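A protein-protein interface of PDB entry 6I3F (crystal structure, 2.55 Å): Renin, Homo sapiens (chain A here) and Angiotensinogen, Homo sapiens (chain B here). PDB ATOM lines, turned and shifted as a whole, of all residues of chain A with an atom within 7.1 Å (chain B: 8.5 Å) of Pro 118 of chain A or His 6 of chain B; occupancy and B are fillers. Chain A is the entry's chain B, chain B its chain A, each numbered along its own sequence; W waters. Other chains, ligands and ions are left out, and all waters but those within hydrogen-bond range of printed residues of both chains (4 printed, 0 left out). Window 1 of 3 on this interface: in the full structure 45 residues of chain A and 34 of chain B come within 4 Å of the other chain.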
ATOM      1  N   TYR A  15      18.880   9.281   9.554  1.00  0.00           N
ATOM      2  CA  TYR A  15      19.745   9.137   8.355  1.00  0.00           C
ATOM      3  C   TYR A  15      19.753  10.461   7.582  1.00  0.00           C
ATOM      4  O   TYR A  15      18.725  10.794   6.961  1.00  0.00           O
ATOM      5  CB  TYR A  15      19.265   7.982   7.474  1.00  0.00           C
ATOM      6  CG  TYR A  15      20.036   7.833   6.187  1.00  0.00           C
ATOM      7  CD1 TYR A  15      21.252   7.170   6.158  1.00  0.00           C
ATOM      8  CD2 TYR A  15      19.564   8.373   5.002  1.00  0.00           C
ATOM      9  CE1 TYR A  15      21.975   7.036   4.983  1.00  0.00           C
ATOM     10  CE2 TYR A  15      20.274   8.251   3.819  1.00  0.00           C
ATOM     11  CZ  TYR A  15      21.485   7.579   3.810  1.00  0.00           C
ATOM     12  OH  TYR A  15      22.194   7.451   2.650  1.00  0.00           O
ATOM     13  N   THR A  18      17.079  13.379   6.861  1.00  0.00           N
ATOM     14  CA  THR A  18      16.037  13.219   5.804  1.00  0.00           C
ATOM     15  C   THR A  18      15.135  12.004   6.068  1.00  0.00           C
ATOM     16  O   THR A  18      13.968  12.054   5.633  1.00  0.00           O
ATOM     17  CB  THR A  18      16.668  13.111   4.411  1.00  0.00           C
ATOM     18  OG1 THR A  18      17.649  12.076   4.451  1.00  0.00           O
ATOM     19  CG2 THR A  18      17.293  14.409   3.953  1.00  0.00           C
ATOM     20  N   GLN A  19      15.644  10.948   6.714  1.00  0.00           N
ATOM     21  CA  GLN A  19      14.878   9.699   6.978  1.00  0.00           C
ATOM     22  C   GLN A  19      14.974   9.340   8.465  1.00  0.00           C
ATOM     23  O   GLN A  19      16.028   8.827   8.886  1.00  0.00           O
ATOM     24  CB  GLN A  19      15.393   8.562   6.095  1.00  0.00           C
ATOM     25  CG  GLN A  19      15.328   8.866   4.605  1.00  0.00           C
ATOM     26  CD  GLN A  19      15.896   7.744   3.770  1.00  0.00           C
ATOM     27  OE1 GLN A  19      15.713   6.567   4.074  1.00  0.00           O
ATOM     28  NE2 GLN A  19      16.593   8.104   2.705  1.00  0.00           N
ATOM     29  N   ALA A  57      14.398  -2.565  -6.013  1.00  0.00           N
ATOM     30  CA  ALA A  57      13.971  -1.907  -4.754  1.00  0.00           C
ATOM     31  C   ALA A  57      13.436  -2.938  -3.749  1.00  0.00           C
ATOM     32  O   ALA A  57      13.629  -2.721  -2.543  1.00  0.00           O
ATOM     33  CB  ALA A  57      12.944  -0.841  -5.054  1.00  0.00           C
ATOM     34  N   TYR A  83       2.450   8.592  -5.494  1.00  0.00           N
ATOM     35  CA  TYR A  83       3.281   9.716  -4.984  1.00  0.00           C
ATOM     36  C   TYR A  83       3.613  10.637  -6.166  1.00  0.00           C
ATOM     37  O   TYR A  83       3.145  10.348  -7.284  1.00  0.00           O
ATOM     38  CB  TYR A  83       4.514   9.173  -4.256  1.00  0.00           C
ATOM     39  CG  TYR A  83       4.194   8.302  -3.067  1.00  0.00           C
ATOM     40  CD1 TYR A  83       3.727   8.853  -1.885  1.00  0.00           C
ATOM     41  CD2 TYR A  83       4.343   6.925  -3.124  1.00  0.00           C
ATOM     42  CE1 TYR A  83       3.421   8.061  -0.789  1.00  0.00           C
ATOM     43  CE2 TYR A  83       4.042   6.119  -2.036  1.00  0.00           C
ATOM     44  CZ  TYR A  83       3.579   6.688  -0.863  1.00  0.00           C
ATOM     45  OH  TYR A  83       3.278   5.904   0.214  1.00  0.00           O
ATOM     46  N   SER A  84       4.380  11.707  -5.926  1.00  0.00           N
ATOM     47  CA  SER A  84       4.670  12.785  -6.910  1.00  0.00           C
ATOM     48  C   SER A  84       5.301  12.203  -8.184  1.00  0.00           C
ATOM     49  O   SER A  84       4.744  12.436  -9.277  1.00  0.00           O
ATOM     50  CB  SER A  84       5.539  13.858  -6.304  1.00  0.00           C
ATOM     51  OG  SER A  84       6.844  13.370  -6.031  1.00  0.00           O
ATOM     52  N   THR A  85       6.412  11.470  -8.045  1.00  0.00           N
ATOM     53  CA  THR A  85       7.225  10.930  -9.170  1.00  0.00           C
ATOM     54  C   THR A  85       6.803   9.489  -9.482  1.00  0.00           C
ATOM     55  O   THR A  85       6.461   9.218 -10.652  1.00  0.00           O
ATOM     56  CB  THR A  85       8.725  11.000  -8.855  1.00  0.00           C
ATOM     57  OG1 THR A  85       8.972  10.209  -7.691  1.00  0.00           O
ATOM     58  CG2 THR A  85       9.215  12.415  -8.632  1.00  0.00           C
ATOM     59  N   GLY A  86       6.834   8.610  -8.473  1.00  0.00           N
ATOM     60  CA  GLY A  86       6.626   7.155  -8.620  1.00  0.00           C
ATOM     61  C   GLY A  86       5.394   6.660  -7.879  1.00  0.00           C
ATOM     62  O   GLY A  86       4.810   7.436  -7.099  1.00  0.00           O
ATOM     63  N   THR A  87       5.033   5.393  -8.111  1.00  0.00           N
ATOM     64  CA  THR A  87       3.844   4.701  -7.546  1.00  0.00           C
ATOM     65  C   THR A  87       4.268   3.321  -7.033  1.00  0.00           C
ATOM     66  O   THR A  87       4.978   2.621  -7.777  1.00  0.00           O
ATOM     67  CB  THR A  87       2.744   4.584  -8.610  1.00  0.00           C
ATOM     68  OG1 THR A  87       2.288   5.905  -8.903  1.00  0.00           O
ATOM     69  CG2 THR A  87       1.574   3.724  -8.185  1.00  0.00           C
ATOM     70  N   VAL A  88       3.858   2.951  -5.815  1.00  0.00           N
ATOM     71  CA  VAL A  88       3.959   1.556  -5.289  1.00  0.00           C
ATOM     72  C   VAL A  88       2.552   0.953  -5.309  1.00  0.00           C
ATOM     73  O   VAL A  88       1.588   1.692  -5.027  1.00  0.00           O
ATOM     74  CB  VAL A  88       4.601   1.487  -3.886  1.00  0.00           C
ATOM     75  CG1 VAL A  88       5.814   2.397  -3.776  1.00  0.00           C
ATOM     76  CG2 VAL A  88       3.616   1.785  -2.767  1.00  0.00           C
ATOM     77  N   PRO A 115       9.152   1.101  -7.727  1.00  0.00           N
ATOM     78  CA  PRO A 115      10.095   1.738  -8.645  1.00  0.00           C
ATOM     79  C   PRO A 115      11.434   2.010  -7.942  1.00  0.00           C
ATOM     80  O   PRO A 115      11.420   2.384  -6.781  1.00  0.00           O
ATOM     81  CB  PRO A 115       9.383   3.038  -9.045  1.00  0.00           C
ATOM     82  CG  PRO A 115       8.503   3.363  -7.854  1.00  0.00           C
ATOM     83  CD  PRO A 115       8.097   2.022  -7.275  1.00  0.00           C
ATOM     84  N   ALA A 116      12.546   1.804  -8.653  1.00  0.00           N
ATOM     85  CA  ALA A 116      13.925   2.019  -8.153  1.00  0.00           C
ATOM     86  C   ALA A 116      14.043   3.434  -7.576  1.00  0.00           C
ATOM     87  O   ALA A 116      14.676   3.595  -6.519  1.00  0.00           O
ATOM     88  CB  ALA A 116      14.919   1.791  -9.266  1.00  0.00           C
ATOM     89  N   LEU A 117      13.440   4.413  -8.254  1.00  0.00           N
ATOM     90  CA  LEU A 117      13.429   5.844  -7.852  1.00  0.00           C
ATOM     91  C   LEU A 117      12.040   6.176  -7.304  1.00  0.00           C
ATOM     92  O   LEU A 117      11.044   5.971  -7.997  1.00  0.00           O
ATOM     93  CB  LEU A 117      13.786   6.683  -9.087  1.00  0.00           C
ATOM     94  CG  LEU A 117      14.611   7.948  -8.847  1.00  0.00           C
ATOM     95  CD1 LEU A 117      15.847   7.666  -8.004  1.00  0.00           C
ATOM     96  CD2 LEU A 117      15.017   8.576 -10.172  1.00  0.00           C
ATOM     97  N   PRO A 118      11.902   6.687  -6.056  1.00  0.00           N
ATOM     98  CA  PRO A 118      13.029   7.054  -5.194  1.00  0.00           C
ATOM     99  C   PRO A 118      13.487   6.019  -4.153  1.00  0.00           C
ATOM    100  O   PRO A 118      14.352   6.346  -3.362  1.00  0.00           O
ATOM    101  CB  PRO A 118      12.405   8.242  -4.448  1.00  0.00           C
ATOM    102  CG  PRO A 118      10.988   7.781  -4.182  1.00  0.00           C
ATOM    103  CD  PRO A 118      10.611   6.979  -5.412  1.00  0.00           C
ATOM    104  N   PHE A 119      12.921   4.808  -4.175  1.00  0.00           N
ATOM    105  CA  PHE A 119      12.933   3.861  -3.025  1.00  0.00           C
ATOM    106  C   PHE A 119      14.293   3.169  -2.860  1.00  0.00           C
ATOM    107  O   PHE A 119      14.529   2.652  -1.754  1.00  0.00           O
ATOM    108  CB  PHE A 119      11.770   2.871  -3.139  1.00  0.00           C
ATOM    109  CG  PHE A 119      10.440   3.498  -2.812  1.00  0.00           C
ATOM    110  CD1 PHE A 119      10.121   3.834  -1.505  1.00  0.00           C
ATOM    111  CD2 PHE A 119       9.527   3.796  -3.811  1.00  0.00           C
ATOM    112  CE1 PHE A 119       8.909   4.434  -1.201  1.00  0.00           C
ATOM    113  CE2 PHE A 119       8.314   4.397  -3.505  1.00  0.00           C
ATOM    114  CZ  PHE A 119       8.007   4.711  -2.202  1.00  0.00           C
ATOM    115  N   MET A 120      15.169   3.186  -3.872  1.00  0.00           N
ATOM    116  CA  MET A 120      16.554   2.647  -3.745  1.00  0.00           C
ATOM    117  C   MET A 120      17.423   3.624  -2.939  1.00  0.00           C
ATOM    118  O   MET A 120      18.547   3.231  -2.572  1.00  0.00           O
ATOM    119  CB  MET A 120      17.204   2.383  -5.108  1.00  0.00           C
ATOM    120  CG  MET A 120      16.856   1.021  -5.696  1.00  0.00           C
ATOM    121  SD  MET A 120      17.244  -0.374  -4.593  1.00  0.00           S
ATOM    122  CE  MET A 120      19.010  -0.165  -4.376  1.00  0.00           C
ATOM    123  N   LEU A 121      16.927   4.837  -2.669  1.00  0.00           N
ATOM    124  CA  LEU A 121      17.591   5.844  -1.797  1.00  0.00           C
ATOM    125  C   LEU A 121      16.993   5.790  -0.385  1.00  0.00           C
ATOM    126  O   LEU A 121      17.461   6.559   0.476  1.00  0.00           O
ATOM    127  CB  LEU A 121      17.415   7.236  -2.415  1.00  0.00           C
ATOM    128  CG  LEU A 121      17.940   7.393  -3.843  1.00  0.00           C
ATOM    129  CD1 LEU A 121      17.528   8.734  -4.430  1.00  0.00           C
ATOM    130  CD2 LEU A 121      19.453   7.235  -3.889  1.00  0.00           C
ATOM    131  N   ALA A 122      16.010   4.911  -0.155  1.00  0.00           N
ATOM    132  CA  ALA A 122      15.308   4.732   1.139  1.00  0.00           C
ATOM    133  C   ALA A 122      16.062   3.719   2.010  1.00  0.00           C
ATOM    134  O   ALA A 122      16.249   2.576   1.560  1.00  0.00           O
ATOM    135  CB  ALA A 122      13.883   4.293   0.899  1.00  0.00           C
ATOM    136  N   PHE A 124      14.691   3.033   4.949  1.00  0.00           N
ATOM    137  CA  PHE A 124      13.456   2.386   5.466  1.00  0.00           C
ATOM    138  C   PHE A 124      12.952   1.369   4.435  1.00  0.00           C
ATOM    139  O   PHE A 124      13.277   1.500   3.241  1.00  0.00           O
ATOM    140  CB  PHE A 124      12.392   3.435   5.812  1.00  0.00           C
ATOM    141  CG  PHE A 124      11.909   4.277   4.657  1.00  0.00           C
ATOM    142  CD1 PHE A 124      12.483   5.509   4.385  1.00  0.00           C
ATOM    143  CD2 PHE A 124      10.867   3.845   3.849  1.00  0.00           C
ATOM    144  CE1 PHE A 124      12.035   6.287   3.328  1.00  0.00           C
ATOM    145  CE2 PHE A 124      10.422   4.623   2.789  1.00  0.00           C
ATOM    146  CZ  PHE A 124      11.006   5.841   2.531  1.00  0.00           C
ATOM    147  N   SER A 230      10.807  14.955   4.478  1.00  0.00           N
ATOM    148  CA  SER A 230      12.193  15.327   4.866  1.00  0.00           C
ATOM    149  C   SER A 230      12.278  16.841   5.072  1.00  0.00           C
ATOM    150  O   SER A 230      12.736  17.272   6.148  1.00  0.00           O
ATOM    151  CB  SER A 230      13.195  14.872   3.834  1.00  0.00           C
ATOM    152  OG  SER A 230      13.168  13.462   3.674  1.00  0.00           O
ATOM    153  N   TYR A 231      11.848  17.608   4.067  1.00  0.00           N
ATOM    154  CA  TYR A 231      11.974  19.086   4.007  1.00  0.00           C
ATOM    155  C   TYR A 231      10.650  19.753   4.392  1.00  0.00           C
ATOM    156  O   TYR A 231       9.633  19.060   4.579  1.00  0.00           O
ATOM    157  CB  TYR A 231      12.369  19.540   2.598  1.00  0.00           C
ATOM    158  CG  TYR A 231      13.756  19.167   2.131  1.00  0.00           C
ATOM    159  CD1 TYR A 231      14.690  18.584   2.976  1.00  0.00           C
ATOM    160  CD2 TYR A 231      14.151  19.448   0.832  1.00  0.00           C
ATOM    161  CE1 TYR A 231      15.965  18.261   2.533  1.00  0.00           C
ATOM    162  CE2 TYR A 231      15.420  19.136   0.376  1.00  0.00           C
ATOM    163  CZ  TYR A 231      16.331  18.540   1.229  1.00  0.00           C
ATOM    164  OH  TYR A 231      17.580  18.228   0.778  1.00  0.00           O
ATOM    165  N   PHE A 253      18.545  19.032  -8.656  1.00  0.00           N
ATOM    166  CA  PHE A 253      17.288  18.787  -7.901  1.00  0.00           C
ATOM    167  C   PHE A 253      17.201  19.729  -6.696  1.00  0.00           C
ATOM    168  O   PHE A 253      16.076  20.003  -6.243  1.00  0.00           O
ATOM    169  CB  PHE A 253      17.212  17.334  -7.429  1.00  0.00           C
ATOM    170  CG  PHE A 253      17.328  16.308  -8.528  1.00  0.00           C
ATOM    171  CD1 PHE A 253      16.253  16.035  -9.360  1.00  0.00           C
ATOM    172  CD2 PHE A 253      18.512  15.612  -8.725  1.00  0.00           C
ATOM    173  CE1 PHE A 253      16.361  15.091 -10.370  1.00  0.00           C
ATOM    174  CE2 PHE A 253      18.618  14.669  -9.735  1.00  0.00           C
ATOM    175  CZ  PHE A 253      17.543  14.409 -10.555  1.00  0.00           C
ATOM    176  N   ASP A 254      18.350  20.197  -6.203  1.00  0.00           N
ATOM    177  CA  ASP A 254      18.475  20.970  -4.939  1.00  0.00           C
ATOM    178  C   ASP A 254      18.318  22.466  -5.218  1.00  0.00           C
ATOM    179  O   ASP A 254      18.583  22.893  -6.357  1.00  0.00           O
ATOM    180  CB  ASP A 254      19.828  20.717  -4.271  1.00  0.00           C
ATOM    181  CG  ASP A 254      20.072  19.260  -3.924  1.00  0.00           C
ATOM    182  OD1 ASP A 254      19.221  18.671  -3.225  1.00  0.00           O
ATOM    183  OD2 ASP A 254      21.107  18.724  -4.364  1.00  0.00           O
ATOM    184  N   HIS A 301      11.911  22.614  -0.439  1.00  0.00           N
ATOM    185  CA  HIS A 301      11.686  22.278  -1.872  1.00  0.00           C
ATOM    186  C   HIS A 301      10.217  22.500  -2.251  1.00  0.00           C
ATOM    187  O   HIS A 301       9.416  22.817  -1.357  1.00  0.00           O
ATOM    188  CB  HIS A 301      12.174  20.853  -2.177  1.00  0.00           C
ATOM    189  CG  HIS A 301      11.341  19.763  -1.588  1.00  0.00           C
ATOM    190  ND1 HIS A 301      11.187  18.539  -2.211  1.00  0.00           N
ATOM    191  CD2 HIS A 301      10.621  19.697  -0.445  1.00  0.00           C
ATOM    192  CE1 HIS A 301      10.411  17.768  -1.477  1.00  0.00           C
ATOM    193  NE2 HIS A 301      10.050  18.456  -0.387  1.00  0.00           N
ATOM    194  N   VAL B   3      27.322  13.828  -3.869  1.00  0.00           N
ATOM    195  CA  VAL B   3      26.243  12.795  -3.803  1.00  0.00           C
ATOM    196  C   VAL B   3      24.909  13.480  -3.474  1.00  0.00           C
ATOM    197  O   VAL B   3      24.886  14.365  -2.595  1.00  0.00           O
ATOM    198  CB  VAL B   3      26.579  11.688  -2.784  1.00  0.00           C
ATOM    199  CG1 VAL B   3      25.392  10.770  -2.517  1.00  0.00           C
ATOM    200  CG2 VAL B   3      27.789  10.877  -3.222  1.00  0.00           C
ATOM    201  N   TYR B   4      23.842  13.056  -4.155  1.00  0.00           N
ATOM    202  CA  TYR B   4      22.454  13.564  -4.003  1.00  0.00           C
ATOM    203  C   TYR B   4      21.782  12.865  -2.816  1.00  0.00           C
ATOM    204  O   TYR B   4      21.758  11.620  -2.785  1.00  0.00           O
ATOM    205  CB  TYR B   4      21.684  13.346  -5.308  1.00  0.00           C
ATOM    206  CG  TYR B   4      20.197  13.581  -5.230  1.00  0.00           C
ATOM    207  CD1 TYR B   4      19.684  14.844  -4.983  1.00  0.00           C
ATOM    208  CD2 TYR B   4      19.299  12.544  -5.427  1.00  0.00           C
ATOM    209  CE1 TYR B   4      18.318  15.069  -4.920  1.00  0.00           C
ATOM    210  CE2 TYR B   4      17.930  12.752  -5.370  1.00  0.00           C
ATOM    211  CZ  TYR B   4      17.437  14.020  -5.117  1.00  0.00           C
ATOM    212  OH  TYR B   4      16.090  14.237  -5.060  1.00  0.00           O
ATOM    213  N   ILE B   5      21.268  13.654  -1.866  1.00  0.00           N
ATOM    214  CA  ILE B   5      20.452  13.192  -0.702  1.00  0.00           C
ATOM    215  C   ILE B   5      18.983  13.524  -0.996  1.00  0.00           C
ATOM    216  O   ILE B   5      18.631  14.715  -0.948  1.00  0.00           O
ATOM    217  CB  ILE B   5      20.935  13.850   0.610  1.00  0.00           C
ATOM    218  CG1 ILE B   5      22.455  13.759   0.785  1.00  0.00           C
ATOM    219  CG2 ILE B   5      20.198  13.268   1.807  1.00  0.00           C
ATOM    220  CD1 ILE B   5      22.997  12.346   0.821  1.00  0.00           C
ATOM    221  N   HIS B   6      18.163  12.514  -1.301  1.00  0.00           N
ATOM    222  CA  HIS B   6      16.751  12.690  -1.738  1.00  0.00           C
ATOM    223  C   HIS B   6      15.881  13.072  -0.545  1.00  0.00           C
ATOM    224  O   HIS B   6      15.834  12.348   0.447  1.00  0.00           O
ATOM    225  CB  HIS B   6      16.214  11.436  -2.441  1.00  0.00           C
ATOM    226  CG  HIS B   6      14.784  11.559  -2.853  1.00  0.00           C
ATOM    227  ND1 HIS B   6      14.391  12.304  -3.947  1.00  0.00           N
ATOM    228  CD2 HIS B   6      13.653  11.050  -2.316  1.00  0.00           C
ATOM    229  CE1 HIS B   6      13.081  12.242  -4.073  1.00  0.00           C
ATOM    230  NE2 HIS B   6      12.603  11.478  -3.084  1.00  0.00           N
ATOM    231  N   PRO B   7      15.164  14.219  -0.610  1.00  0.00           N
ATOM    232  CA  PRO B   7      14.163  14.564   0.396  1.00  0.00           C
ATOM    233  C   PRO B   7      12.855  13.818   0.108  1.00  0.00           C
ATOM    234  O   PRO B   7      12.269  14.053  -0.929  1.00  0.00           O
ATOM    235  CB  PRO B   7      13.991  16.076   0.215  1.00  0.00           C
ATOM    236  CG  PRO B   7      14.268  16.308  -1.261  1.00  0.00           C
ATOM    237  CD  PRO B   7      15.270  15.245  -1.662  1.00  0.00           C
ATOM    238  N   PHE B   8      12.442  12.928   1.013  1.00  0.00           N
ATOM    239  CA  PHE B   8      11.240  12.073   0.835  1.00  0.00           C
ATOM    240  C   PHE B   8       9.992  12.916   1.112  1.00  0.00           C
ATOM    241  O   PHE B   8      10.036  13.798   1.986  1.00  0.00           O
ATOM    242  CB  PHE B   8      11.343  10.804   1.684  1.00  0.00           C
ATOM    243  CG  PHE B   8      12.103   9.694   1.003  1.00  0.00           C
ATOM    244  CD1 PHE B   8      11.442   8.762   0.217  1.00  0.00           C
ATOM    245  CD2 PHE B   8      13.482   9.605   1.114  1.00  0.00           C
ATOM    246  CE1 PHE B   8      12.141   7.753  -0.430  1.00  0.00           C
ATOM    247  CE2 PHE B   8      14.180   8.596   0.468  1.00  0.00           C
ATOM    248  CZ  PHE B   8      13.508   7.672  -0.303  1.00  0.00           C
ATOM    249  N   HIS B   9       8.942  12.685   0.319  1.00  0.00           N
ATOM    250  CA  HIS B   9       7.590  13.282   0.471  1.00  0.00           C
ATOM    251  C   HIS B   9       6.564  12.160   0.301  1.00  0.00           C
ATOM    252  O   HIS B   9       6.359  11.717  -0.847  1.00  0.00           O
ATOM    253  CB  HIS B   9       7.393  14.439  -0.519  1.00  0.00           C
ATOM    254  CG  HIS B   9       6.528  15.533   0.008  1.00  0.00           C
ATOM    255  ND1 HIS B   9       5.172  15.368   0.217  1.00  0.00           N
ATOM    256  CD2 HIS B   9       6.816  16.801   0.373  1.00  0.00           C
ATOM    257  CE1 HIS B   9       4.663  16.489   0.686  1.00  0.00           C
ATOM    258  NE2 HIS B   9       5.651  17.385   0.788  1.00  0.00           N
ATOM    259  N   LEU B  10       5.980  11.700   1.411  1.00  0.00           N
ATOM    260  CA  LEU B  10       5.139  10.475   1.481  1.00  0.00           C
ATOM    261  C   LEU B  10       3.663  10.858   1.637  1.00  0.00           C
ATOM    262  O   LEU B  10       2.860   9.970   1.980  1.00  0.00           O
ATOM    263  CB  LEU B  10       5.630   9.611   2.647  1.00  0.00           C
ATOM    264  CG  LEU B  10       7.075   9.123   2.534  1.00  0.00           C
ATOM    265  CD1 LEU B  10       7.517   8.436   3.817  1.00  0.00           C
ATOM    266  CD2 LEU B  10       7.249   8.192   1.343  1.00  0.00           C
ATOM    267  N   MET B  75      20.881   7.892 -12.153  1.00  0.00           N
ATOM    268  CA  MET B  75      20.637   7.234 -10.839  1.00  0.00           C
ATOM    269  C   MET B  75      20.035   5.839 -11.066  1.00  0.00           C
ATOM    270  O   MET B  75      20.488   4.890 -10.394  1.00  0.00           O
ATOM    271  CB  MET B  75      19.712   8.078  -9.954  1.00  0.00           C
ATOM    272  CG  MET B  75      20.415   9.283  -9.348  1.00  0.00           C
ATOM    273  SD  MET B  75      19.453  10.130  -8.064  1.00  0.00           S
ATOM    274  CE  MET B  75      18.147  10.859  -9.052  1.00  0.00           C
ATOM    275  N   LEU B  76      19.073   5.714 -11.986  1.00  0.00           N
ATOM    276  CA  LEU B  76      18.448   4.417 -12.362  1.00  0.00           C
ATOM    277  C   LEU B  76      19.537   3.438 -12.824  1.00  0.00           C
ATOM    278  O   LEU B  76      19.494   2.263 -12.404  1.00  0.00           O
ATOM    279  CB  LEU B  76      17.408   4.645 -13.465  1.00  0.00           C
ATOM    280  CG  LEU B  76      16.119   5.346 -13.032  1.00  0.00           C
ATOM    281  CD1 LEU B  76      15.249   5.667 -14.238  1.00  0.00           C
ATOM    282  CD2 LEU B  76      15.344   4.505 -12.027  1.00  0.00           C
ATOM    283  N   PHE B  79      21.789   2.007  -9.922  1.00  0.00           N
ATOM    284  CA  PHE B  79      21.095   0.967  -9.117  1.00  0.00           C
ATOM    285  C   PHE B  79      21.191  -0.383  -9.836  1.00  0.00           C
ATOM    286  O   PHE B  79      21.577  -1.379  -9.193  1.00  0.00           O
ATOM    287  CB  PHE B  79      19.639   1.352  -8.844  1.00  0.00           C
ATOM    288  CG  PHE B  79      19.447   2.678  -8.149  1.00  0.00           C
ATOM    289  CD1 PHE B  79      20.300   3.086  -7.132  1.00  0.00           C
ATOM    290  CD2 PHE B  79      18.402   3.515  -8.509  1.00  0.00           C
ATOM    291  CE1 PHE B  79      20.118   4.308  -6.502  1.00  0.00           C
ATOM    292  CE2 PHE B  79      18.223   4.735  -7.877  1.00  0.00           C
ATOM    293  CZ  PHE B  79      19.080   5.130  -6.875  1.00  0.00           C
ATOM    294  N   GLY B 130      13.608  -0.253 -13.751  1.00  0.00           N
ATOM    295  CA  GLY B 130      13.184   0.295 -12.448  1.00  0.00           C
ATOM    296  C   GLY B 130      12.288   1.515 -12.582  1.00  0.00           C
ATOM    297  O   GLY B 130      12.053   2.176 -11.550  1.00  0.00           O
HETATM  298  O   HOH W   1      17.377  10.676   1.968  1.00  0.00           O
HETATM  299  O   HOH W   2       2.787   7.250   2.435  1.00  0.00           O
HETATM  300  O   HOH W   3      10.101  16.669   1.888  1.00  0.00           O
HETATM  301  O   HOH W   4       5.442  12.501  -3.356  1.00  0.00           O
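The side-chain hydroxyl (OH) of Tyr 4 of chain B lies within hydrogen-bond range of a ring nitrogen (ND1) of His 6 of chain B, 2.8 Å away.
OG1 of Thr 18 of chain A lies within hydrogen-bond range of O of Tyr 15 of chain A, at 3.0 Å.
O of Thr 18 of chain A sits at hydrogen-bond distance from OG of Ser 230 of chain A (2.5 Å).
The backbone carbonyl oxygen (O) of Leu 121 of chain A lies within hydrogen-bond range of the side-chain amide nitrogen (NE2) of Gln 19 of chain A, at 2.8 Å.
Of chain B, only His 6 and Phe 8 come within 4 Å of Pro 118 of chain A.
Of chain A, only Pro 118 (3.5 Å) and Leu 121 (3.6 Å) come within 4 Å of His 6 of chain B.
Printed residues of chain B within 4 Å of Thr 18 of chain A: Ile 5 (3.8 Å).
Of the printed residues of chain B, Tyr 231 of chain A touches Pro 7.
Of the printed residues of chain A, Gly 130 of chain B touches Pro 115 (3.5 Å) and Ala 116 (3.0 Å).
Printed residues of chain B within 4 Å of Ala 116 of chain A: Leu 76 (3.9 Å), Phe 79 (3.96 Å) and Gly 130 (3.0 Å).
Val 3 of chain B touches none of the printed residues of chain A.
The nearest residue of chain A that does not touch His 6 of chain B is Thr 18 of chain A (4.1 Å).
Ile 5 of chain B touches Thr 18 of chain A.
O of Leu 10 of chain B touches CE1 of Tyr 83 of chain A, 3.4 Å away.
Pro 115 of chain A touches Gly 130 of chain B (CA to O, 3.5 Å).
Phe 79 of chain B touches Ala 116 of chain A (CD2 to CB, 3.96 Å).
Phe 79 of chain B touches Leu 117 of chain A.
CB of Met 120 of chain A touches CE1 of Phe 79 of chain B (3.8 Å).
Leu 121 of chain A touches His 6 of chain B.
CZ of Phe 124 of chain A touches CE1 of Phe 8 of chain B, at 3.7 Å.
CE2 of Phe 253 of chain A touches CE of Met 75 of chain B, 3.9 Å away.
His 301 of chain A touches Pro 7 of chain B (ND1 to CG, 3.9 Å).
The backbone NH of Phe 8 of chain B sits at hydrogen-bond distance from the side-chain hydroxyl of Ser 230 of chain A, at 2.8 Å.
The backbone NH (N) of Ala 116 of chain A sits at hydrogen-bond distance from the backbone carbonyl oxygen (O) of Gly 130 of chain B, 3.0 Å away.
Of the 24 printed residues of chain A, 15 touch a printed residue of chain B.
Printed residues of chain A that touch a printed residue of chain B: Thr 18, Gln 19, Tyr 83, Pro 115, Ala 116, Leu 117, Pro 118, Met 120, Leu 121, Ala 122, Phe 124, Ser 230, Tyr 231, Phe 253 and His 301.
Hydrophobic or aromatic side chains of chain A within 4 Å of the printed part of chain B: Tyr 83, Pro 115, Ala 116, Leu 117, Pro 118, Met 120, Leu 121, Ala 122, Phe 124, Tyr 231, Phe 253 and His 301.
Among the printed residues, 24 pairs touch across the chains.
Among the printed residues, no Asp or Glu carboxylate lies within 4 Å of a Lys or Arg side-chain nitrogen of the other chain.
Water W2 lies within hydrogen-bond range of the side-chain hydroxyl (OH) of Tyr 83 of chain A (2.6 Å) and the backbone carbonyl oxygen (O) of Leu 10 of chain B (2.8 Å).
Water W1 lies within hydrogen-bond range of the backbone carbonyl oxygen (O) of His 6 of chain B, the side-chain amide nitrogen (NE2) of Gln 19 of chain A and the side-chain hydroxyl (OG1) of Thr 18 of chain A.
Water W4 lies within hydrogen-bond range of O of His 9 of chain B and N of Ser 84 of chain A.
Water W3 lies within hydrogen-bond range of O of Phe 8 of chain B, NE2 of His 301 of chain A, N of Tyr 231 of chain A and N of Ser 230 of chain A.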
